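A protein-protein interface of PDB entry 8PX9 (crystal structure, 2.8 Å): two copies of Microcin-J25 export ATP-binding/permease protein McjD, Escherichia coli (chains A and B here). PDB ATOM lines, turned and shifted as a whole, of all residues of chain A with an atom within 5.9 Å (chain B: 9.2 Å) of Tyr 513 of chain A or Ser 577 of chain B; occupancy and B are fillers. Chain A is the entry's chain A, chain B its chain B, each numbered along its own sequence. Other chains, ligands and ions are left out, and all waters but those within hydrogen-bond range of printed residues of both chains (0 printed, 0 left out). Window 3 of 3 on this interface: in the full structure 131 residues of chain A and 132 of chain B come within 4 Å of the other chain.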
ATOM      1  N   LEU A 511      12.041 -36.847 -13.295  1.00  0.00           N
ATOM      2  CA  LEU A 511      12.184 -36.013 -14.500  1.00  0.00           C
ATOM      3  C   LEU A 511      13.167 -34.865 -14.205  1.00  0.00           C
ATOM      4  O   LEU A 511      13.156 -34.301 -13.104  1.00  0.00           O
ATOM      5  CB  LEU A 511      10.824 -35.402 -14.910  1.00  0.00           C
ATOM      6  CG  LEU A 511       9.715 -36.366 -15.340  1.00  0.00           C
ATOM      7  CD1 LEU A 511       8.464 -35.602 -15.723  1.00  0.00           C
ATOM      8  CD2 LEU A 511      10.149 -37.280 -16.485  1.00  0.00           C
ATOM      9  N   ASP A 512      13.993 -34.470 -15.202  1.00  0.00           N
ATOM     10  CA  ASP A 512      14.877 -33.299 -15.089  1.00  0.00           C
ATOM     11  C   ASP A 512      14.057 -32.013 -15.203  1.00  0.00           C
ATOM     12  O   ASP A 512      12.937 -32.044 -15.720  1.00  0.00           O
ATOM     13  CB  ASP A 512      16.019 -33.332 -16.115  1.00  0.00           C
ATOM     14  CG  ASP A 512      15.566 -33.262 -17.572  1.00  0.00           C
ATOM     15  OD1 ASP A 512      14.459 -33.798 -17.884  1.00  0.00           O
ATOM     16  OD2 ASP A 512      16.315 -32.695 -18.398  1.00  0.00           O
ATOM     17  N   TYR A 513      14.632 -30.875 -14.761  1.00  0.00           N
ATOM     18  CA  TYR A 513      13.947 -29.565 -14.732  1.00  0.00           C
ATOM     19  C   TYR A 513      13.280 -29.169 -16.071  1.00  0.00           C
ATOM     20  O   TYR A 513      12.180 -28.585 -16.050  1.00  0.00           O
ATOM     21  CB  TYR A 513      14.863 -28.415 -14.264  1.00  0.00           C
ATOM     22  CG  TYR A 513      14.249 -27.011 -14.250  1.00  0.00           C
ATOM     23  CD1 TYR A 513      13.337 -26.615 -13.267  1.00  0.00           C
ATOM     24  CD2 TYR A 513      14.528 -26.107 -15.284  1.00  0.00           C
ATOM     25  CE1 TYR A 513      12.714 -25.380 -13.339  1.00  0.00           C
ATOM     26  CE2 TYR A 513      13.887 -24.880 -15.356  1.00  0.00           C
ATOM     27  CZ  TYR A 513      12.989 -24.505 -14.375  1.00  0.00           C
ATOM     28  OH  TYR A 513      12.377 -23.279 -14.415  1.00  0.00           O
ATOM     29  N   ILE A 514      13.897 -29.539 -17.206  1.00  0.00           N
ATOM     30  CA  ILE A 514      13.393 -29.235 -18.535  1.00  0.00           C
ATOM     31  C   ILE A 514      12.090 -29.987 -18.813  1.00  0.00           C
ATOM     32  O   ILE A 514      11.082 -29.305 -19.039  1.00  0.00           O
ATOM     33  CB  ILE A 514      14.459 -29.514 -19.633  1.00  0.00           C
ATOM     34  CG1 ILE A 514      15.767 -28.735 -19.404  1.00  0.00           C
ATOM     35  CG2 ILE A 514      13.897 -29.303 -21.050  1.00  0.00           C
ATOM     36  CD1 ILE A 514      15.631 -27.231 -19.299  1.00  0.00           C
ATOM     37  N   ASN A 515      12.088 -31.336 -18.748  1.00  0.00           N
ATOM     38  CA  ASN A 515      10.901 -32.169 -18.944  1.00  0.00           C
ATOM     39  C   ASN A 515       9.812 -31.900 -17.901  1.00  0.00           C
ATOM     40  O   ASN A 515       8.644 -31.800 -18.260  1.00  0.00           O
ATOM     41  CB  ASN A 515      11.244 -33.665 -18.939  1.00  0.00           C
ATOM     42  CG  ASN A 515      11.891 -34.174 -20.205  1.00  0.00           C
ATOM     43  OD1 ASN A 515      11.526 -33.756 -21.304  1.00  0.00           O
ATOM     44  ND2 ASN A 515      12.772 -35.159 -20.061  1.00  0.00           N
ATOM     45  N   GLU A 516      10.197 -31.777 -16.618  1.00  0.00           N
ATOM     46  CA  GLU A 516       9.283 -31.503 -15.506  1.00  0.00           C
ATOM     47  C   GLU A 516       8.467 -30.232 -15.761  1.00  0.00           C
ATOM     48  O   GLU A 516       7.239 -30.316 -15.822  1.00  0.00           O
ATOM     49  CB  GLU A 516      10.049 -31.410 -14.183  1.00  0.00           C
ATOM     50  CG  GLU A 516       9.187 -31.353 -12.944  1.00  0.00           C
ATOM     51  CD  GLU A 516       9.962 -31.110 -11.657  1.00  0.00           C
ATOM     52  OE1 GLU A 516       9.365 -30.760 -10.638  1.00  0.00           O
ATOM     53  OE2 GLU A 516      11.209 -31.284 -11.642  1.00  0.00           O
ATOM     54  N   SER A 517       9.146 -29.100 -15.990  1.00  0.00           N
ATOM     55  CA  SER A 517       8.507 -27.808 -16.254  1.00  0.00           C
ATOM     56  C   SER A 517       7.711 -27.771 -17.569  1.00  0.00           C
ATOM     57  O   SER A 517       6.679 -27.118 -17.639  1.00  0.00           O
ATOM     58  CB  SER A 517       9.533 -26.691 -16.212  1.00  0.00           C
ATOM     59  OG  SER A 517      10.179 -26.655 -14.940  1.00  0.00           O
ATOM     60  N   GLU A 518       8.179 -28.492 -18.592  1.00  0.00           N
ATOM     61  CA  GLU A 518       7.508 -28.586 -19.888  1.00  0.00           C
ATOM     62  C   GLU A 518       6.176 -29.347 -19.772  1.00  0.00           C
ATOM     63  O   GLU A 518       5.185 -28.944 -20.389  1.00  0.00           O
ATOM     64  CB  GLU A 518       8.427 -29.271 -20.908  1.00  0.00           C
ATOM     65  CG  GLU A 518       8.231 -28.824 -22.339  1.00  0.00           C
ATOM     66  CD  GLU A 518       9.320 -29.302 -23.294  1.00  0.00           C
ATOM     67  OE1 GLU A 518      10.530 -29.153 -22.946  1.00  0.00           O
ATOM     68  OE2 GLU A 518       8.970 -29.763 -24.412  1.00  0.00           O
ATOM     69  N   ASN A 540      11.243 -25.687  -6.552  1.00  0.00           N
ATOM     70  CA  ASN A 540      10.777 -25.448  -7.920  1.00  0.00           C
ATOM     71  C   ASN A 540       9.245 -25.545  -8.053  1.00  0.00           C
ATOM     72  O   ASN A 540       8.613 -24.687  -8.673  1.00  0.00           O
ATOM     73  CB  ASN A 540      11.479 -26.419  -8.894  1.00  0.00           C
ATOM     74  CG  ASN A 540      11.015 -26.359 -10.340  1.00  0.00           C
ATOM     75  OD1 ASN A 540      10.749 -25.287 -10.876  1.00  0.00           O
ATOM     76  ND2 ASN A 540      10.929 -27.509 -10.985  1.00  0.00           N
ATOM     77  N   THR B 377      24.819 -37.587 -13.982  1.00  0.00           N
ATOM     78  CA  THR B 377      23.551 -36.996 -14.421  1.00  0.00           C
ATOM     79  C   THR B 377      23.435 -37.068 -15.950  1.00  0.00           C
ATOM     80  O   THR B 377      24.366 -37.510 -16.636  1.00  0.00           O
ATOM     81  CB  THR B 377      23.398 -35.575 -13.848  1.00  0.00           C
ATOM     82  OG1 THR B 377      23.441 -35.648 -12.429  1.00  0.00           O
ATOM     83  CG2 THR B 377      22.082 -34.906 -14.128  1.00  0.00           C
ATOM     84  N   GLY B 378      22.224 -36.759 -16.453  1.00  0.00           N
ATOM     85  CA  GLY B 378      21.912 -36.698 -17.861  1.00  0.00           C
ATOM     86  C   GLY B 378      20.428 -36.935 -18.093  1.00  0.00           C
ATOM     87  O   GLY B 378      19.677 -37.158 -17.129  1.00  0.00           O
ATOM     88  N   PRO B 379      19.952 -36.915 -19.360  1.00  0.00           N
ATOM     89  CA  PRO B 379      18.536 -37.183 -19.650  1.00  0.00           C
ATOM     90  C   PRO B 379      18.113 -38.618 -19.312  1.00  0.00           C
ATOM     91  O   PRO B 379      18.945 -39.421 -18.861  1.00  0.00           O
ATOM     92  CB  PRO B 379      18.406 -36.882 -21.159  1.00  0.00           C
ATOM     93  CG  PRO B 379      19.643 -36.085 -21.495  1.00  0.00           C
ATOM     94  CD  PRO B 379      20.720 -36.638 -20.588  1.00  0.00           C
ATOM     95  N   SER B 536      21.531 -38.129  -9.654  1.00  0.00           N
ATOM     96  CA  SER B 536      20.515 -37.132  -9.323  1.00  0.00           C
ATOM     97  C   SER B 536      20.321 -36.103 -10.445  1.00  0.00           C
ATOM     98  O   SER B 536      21.254 -35.814 -11.168  1.00  0.00           O
ATOM     99  CB  SER B 536      20.896 -36.437  -8.045  1.00  0.00           C
ATOM    100  OG  SER B 536      19.927 -35.473  -7.666  1.00  0.00           O
ATOM    101  N   HIS B 537      19.110 -35.518 -10.530  1.00  0.00           N
ATOM    102  CA  HIS B 537      18.789 -34.388 -11.405  1.00  0.00           C
ATOM    103  C   HIS B 537      18.717 -33.062 -10.633  1.00  0.00           C
ATOM    104  O   HIS B 537      18.362 -32.054 -11.236  1.00  0.00           O
ATOM    105  CB  HIS B 537      17.438 -34.631 -12.101  1.00  0.00           C
ATOM    106  CG  HIS B 537      17.389 -35.830 -12.979  1.00  0.00           C
ATOM    107  ND1 HIS B 537      16.331 -36.710 -12.973  1.00  0.00           N
ATOM    108  CD2 HIS B 537      18.249 -36.280 -13.906  1.00  0.00           C
ATOM    109  CE1 HIS B 537      16.569 -37.662 -13.862  1.00  0.00           C
ATOM    110  NE2 HIS B 537      17.716 -37.408 -14.453  1.00  0.00           N
ATOM    111  N   ARG B 538      19.045 -33.050  -9.322  1.00  0.00           N
ATOM    112  CA  ARG B 538      18.904 -31.904  -8.429  1.00  0.00           C
ATOM    113  C   ARG B 538      20.293 -31.332  -8.127  1.00  0.00           C
ATOM    114  O   ARG B 538      21.245 -32.092  -7.929  1.00  0.00           O
ATOM    115  CB  ARG B 538      18.232 -32.314  -7.112  1.00  0.00           C
ATOM    116  CG  ARG B 538      16.763 -32.697  -7.214  1.00  0.00           C
ATOM    117  CD  ARG B 538      16.205 -33.063  -5.845  1.00  0.00           C
ATOM    118  NE  ARG B 538      16.661 -34.358  -5.354  1.00  0.00           N
ATOM    119  CZ  ARG B 538      16.130 -35.030  -4.323  1.00  0.00           C
ATOM    120  NH1 ARG B 538      15.143 -34.501  -3.611  1.00  0.00           N
ATOM    121  NH2 ARG B 538      16.596 -36.230  -3.990  1.00  0.00           N
ATOM    122  N   ILE B 539      20.373 -29.989  -8.050  1.00  0.00           N
ATOM    123  CA  ILE B 539      21.618 -29.243  -7.861  1.00  0.00           C
ATOM    124  C   ILE B 539      22.250 -29.543  -6.497  1.00  0.00           C
ATOM    125  O   ILE B 539      23.481 -29.632  -6.434  1.00  0.00           O
ATOM    126  CB  ILE B 539      21.357 -27.730  -8.085  1.00  0.00           C
ATOM    127  CG1 ILE B 539      20.978 -27.437  -9.546  1.00  0.00           C
ATOM    128  CG2 ILE B 539      22.494 -26.828  -7.596  1.00  0.00           C
ATOM    129  CD1 ILE B 539      22.002 -27.866 -10.587  1.00  0.00           C
ATOM    130  N   PHE B 562      31.573 -29.171 -10.326  1.00  0.00           N
ATOM    131  CA  PHE B 562      30.224 -28.703 -10.620  1.00  0.00           C
ATOM    132  C   PHE B 562      30.239 -27.266 -11.174  1.00  0.00           C
ATOM    133  O   PHE B 562      29.546 -27.006 -12.149  1.00  0.00           O
ATOM    134  CB  PHE B 562      29.298 -28.874  -9.404  1.00  0.00           C
ATOM    135  CG  PHE B 562      27.953 -28.201  -9.553  1.00  0.00           C
ATOM    136  CD1 PHE B 562      27.005 -28.671 -10.471  1.00  0.00           C
ATOM    137  CD2 PHE B 562      27.649 -27.050  -8.819  1.00  0.00           C
ATOM    138  CE1 PHE B 562      25.781 -28.020 -10.623  1.00  0.00           C
ATOM    139  CE2 PHE B 562      26.429 -26.401  -8.977  1.00  0.00           C
ATOM    140  CZ  PHE B 562      25.503 -26.875  -9.892  1.00  0.00           C
ATOM    141  N   MET B 566      28.775 -26.133 -14.837  1.00  0.00           N
ATOM    142  CA  MET B 566      27.605 -25.262 -14.710  1.00  0.00           C
ATOM    143  C   MET B 566      27.452 -24.306 -15.894  1.00  0.00           C
ATOM    144  O   MET B 566      26.343 -24.161 -16.412  1.00  0.00           O
ATOM    145  CB  MET B 566      27.707 -24.464 -13.402  1.00  0.00           C
ATOM    146  CG  MET B 566      26.529 -23.583 -13.036  1.00  0.00           C
ATOM    147  SD  MET B 566      26.714 -22.981 -11.320  1.00  0.00           S
ATOM    148  CE  MET B 566      24.997 -22.774 -10.840  1.00  0.00           C
ATOM    149  N   GLU B 570      25.549 -27.940 -21.485  1.00  0.00           N
ATOM    150  CA  GLU B 570      24.186 -27.551 -21.819  1.00  0.00           C
ATOM    151  C   GLU B 570      23.169 -28.181 -20.874  1.00  0.00           C
ATOM    152  O   GLU B 570      22.198 -27.517 -20.499  1.00  0.00           O
ATOM    153  CB  GLU B 570      23.810 -27.984 -23.240  1.00  0.00           C
ATOM    154  CG  GLU B 570      24.532 -27.223 -24.331  1.00  0.00           C
ATOM    155  CD  GLU B 570      23.833 -27.232 -25.688  1.00  0.00           C
ATOM    156  OE1 GLU B 570      22.986 -28.144 -25.946  1.00  0.00           O
ATOM    157  OE2 GLU B 570      24.111 -26.302 -26.480  1.00  0.00           O
ATOM    158  N   TYR B 571      23.357 -29.473 -20.558  1.00  0.00           N
ATOM    159  CA  TYR B 571      22.429 -30.204 -19.718  1.00  0.00           C
ATOM    160  C   TYR B 571      22.414 -29.614 -18.303  1.00  0.00           C
ATOM    161  O   TYR B 571      21.322 -29.365 -17.781  1.00  0.00           O
ATOM    162  CB  TYR B 571      22.723 -31.711 -19.752  1.00  0.00           C
ATOM    163  CG  TYR B 571      21.752 -32.485 -18.876  1.00  0.00           C
ATOM    164  CD1 TYR B 571      20.461 -32.801 -19.309  1.00  0.00           C
ATOM    165  CD2 TYR B 571      22.096 -32.812 -17.565  1.00  0.00           C
ATOM    166  CE1 TYR B 571      19.560 -33.447 -18.472  1.00  0.00           C
ATOM    167  CE2 TYR B 571      21.178 -33.397 -16.734  1.00  0.00           C
ATOM    168  CZ  TYR B 571      19.929 -33.750 -17.167  1.00  0.00           C
ATOM    169  OH  TYR B 571      19.169 -34.377 -16.237  1.00  0.00           O
ATOM    170  N   ILE B 572      23.601 -29.398 -17.701  1.00  0.00           N
ATOM    171  CA  ILE B 572      23.721 -28.837 -16.352  1.00  0.00           C
ATOM    172  C   ILE B 572      23.236 -27.376 -16.324  1.00  0.00           C
ATOM    173  O   ILE B 572      22.756 -26.925 -15.286  1.00  0.00           O
ATOM    174  CB  ILE B 572      25.153 -29.038 -15.790  1.00  0.00           C
ATOM    175  CG1 ILE B 572      25.452 -30.533 -15.602  1.00  0.00           C
ATOM    176  CG2 ILE B 572      25.418 -28.274 -14.484  1.00  0.00           C
ATOM    177  CD1 ILE B 572      26.885 -30.879 -15.161  1.00  0.00           C
ATOM    178  N   SER B 573      23.386 -26.624 -17.434  1.00  0.00           N
ATOM    179  CA  SER B 573      22.834 -25.276 -17.573  1.00  0.00           C
ATOM    180  C   SER B 573      21.303 -25.270 -17.496  1.00  0.00           C
ATOM    181  O   SER B 573      20.735 -24.355 -16.904  1.00  0.00           O
ATOM    182  CB  SER B 573      23.315 -24.615 -18.846  1.00  0.00           C
ATOM    183  OG  SER B 573      22.915 -23.254 -18.914  1.00  0.00           O
ATOM    184  N   GLY B 574      20.654 -26.272 -18.114  1.00  0.00           N
ATOM    185  CA  GLY B 574      19.217 -26.485 -18.000  1.00  0.00           C
ATOM    186  C   GLY B 574      18.716 -26.794 -16.582  1.00  0.00           C
ATOM    187  O   GLY B 574      17.565 -26.509 -16.288  1.00  0.00           O
ATOM    188  N   LEU B 575      19.556 -27.431 -15.754  1.00  0.00           N
ATOM    189  CA  LEU B 575      19.277 -27.721 -14.350  1.00  0.00           C
ATOM    190  C   LEU B 575      19.448 -26.456 -13.497  1.00  0.00           C
ATOM    191  O   LEU B 575      18.654 -26.235 -12.587  1.00  0.00           O
ATOM    192  CB  LEU B 575      20.233 -28.817 -13.858  1.00  0.00           C
ATOM    193  CG  LEU B 575      20.249 -30.160 -14.603  1.00  0.00           C
ATOM    194  CD1 LEU B 575      21.409 -31.055 -14.129  1.00  0.00           C
ATOM    195  CD2 LEU B 575      18.907 -30.881 -14.499  1.00  0.00           C
ATOM    196  N   ALA B 576      20.498 -25.646 -13.781  1.00  0.00           N
ATOM    197  CA  ALA B 576      20.833 -24.408 -13.064  1.00  0.00           C
ATOM    198  C   ALA B 576      19.832 -23.252 -13.248  1.00  0.00           C
ATOM    199  O   ALA B 576      19.925 -22.259 -12.518  1.00  0.00           O
ATOM    200  CB  ALA B 576      22.229 -23.949 -13.458  1.00  0.00           C
ATOM    201  N   SER B 577      18.898 -23.344 -14.217  1.00  0.00           N
ATOM    202  CA  SER B 577      17.851 -22.353 -14.457  1.00  0.00           C
ATOM    203  C   SER B 577      16.681 -22.372 -13.458  1.00  0.00           C
ATOM    204  O   SER B 577      15.813 -21.502 -13.581  1.00  0.00           O
ATOM    205  CB  SER B 577      17.343 -22.506 -15.884  1.00  0.00           C
ATOM    206  OG  SER B 577      16.861 -23.825 -16.127  1.00  0.00           O
ATOM    207  N   VAL B 578      16.638 -23.319 -12.491  1.00  0.00           N
ATOM    208  CA  VAL B 578      15.603 -23.391 -11.455  1.00  0.00           C
ATOM    209  C   VAL B 578      15.341 -22.007 -10.846  1.00  0.00           C
ATOM    210  O   VAL B 578      14.193 -21.584 -10.840  1.00  0.00           O
ATOM    211  CB  VAL B 578      15.938 -24.439 -10.365  1.00  0.00           C
ATOM    212  CG1 VAL B 578      15.047 -24.354  -9.119  1.00  0.00           C
ATOM    213  CG2 VAL B 578      15.909 -25.868 -10.908  1.00  0.00           C
ATOM    214  N   THR B 579      16.404 -21.328 -10.381  1.00  0.00           N
ATOM    215  CA  THR B 579      16.352 -19.958  -9.868  1.00  0.00           C
ATOM    216  C   THR B 579      17.030 -19.015 -10.870  1.00  0.00           C
ATOM    217  O   THR B 579      17.837 -19.532 -11.686  1.00  0.00           O
ATOM    218  CB  THR B 579      16.982 -19.879  -8.471  1.00  0.00           C
ATOM    219  OG1 THR B 579      18.344 -20.309  -8.534  1.00  0.00           O
ATOM    220  CG2 THR B 579      16.250 -20.727  -7.450  1.00  0.00           C
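Among the printed residues, merely in contact across the chains: Tyr 513 of chain A with Gly 574 of chain B (3.2 Å), Tyr 513 of chain A with Ser 577 of chain B (3.2 Å), Asp 512 of chain A with Tyr 571 of chain B (3.3 Å), Tyr 513 of chain A with Val 578 of chain B (3.6 Å), Ile 514 of chain A with Gly 574 of chain B (3.7 Å), Leu 511 of chain A with His 537 of chain B (3.9 Å) and Asp 512 of chain A with His 537 of chain B (3.9 Å).
Along chain A the printed residues that touch a printed residue of chain B span positions 511 to 514. Of the 19 printed residues of chain B, 5 touch a printed residue of chain A. Hydrophobic or aromatic side chains of chain B that line the printed part of chain A: His 537, Tyr 571 and Val 578. Along chain B the printed residues that touch a printed residue of chain A span positions 537 to 578. Among the printed residues, 7 pairs touch across the chains.
No position is printed for both chains. Of the 7 pairs that touch across the chains among the printed residues, none has its exchanged pair printed and touching as well.
The side-chain amide nitrogen (ND2) of Asn 515 of chain A sits at hydrogen-bond distance from the side-chain carboxylate (OD1) of Asp 512 of chain A (3.1 Å). O of Tyr 513 of chain A is in hydrogen-bond range of OG of Ser 517 of chain A (3.0 Å). The backbone carbonyl oxygen (O) of Gly 378 of chain B sits at hydrogen-bond distance from a ring nitrogen (NE2) of His 537 of chain B. OH of Tyr 571 of chain B is in hydrogen-bond range of O of Gly 378 of chain B, at 3.0 Å. The side-chain hydroxyl of Ser 577 of chain B is in hydrogen-bond range of the backbone carbonyl oxygen of Gly 574 of chain B (2.8 Å).
Tyr 513 of chain A touches three residues of chain B. Of chain A, only Tyr 513 comes within 4 Å of Ser 577 of chain B. Of chain B, only Gly 574 (3.7 Å) comes within 4 Å of Ile 514 of chain A. Of the printed residues of chain B, Leu 511 of chain A touches His 537 (3.9 Å). Of the printed residues of chain A, Val 578 of chain B touches Tyr 513 (3.6 Å). Of the printed residues of chain A, Gly 574 of chain B touches Tyr 513 and Ile 514. The nearest residue of chain A that does not touch Ser 577 of chain B is Ile 514 of chain A (4.8 Å).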
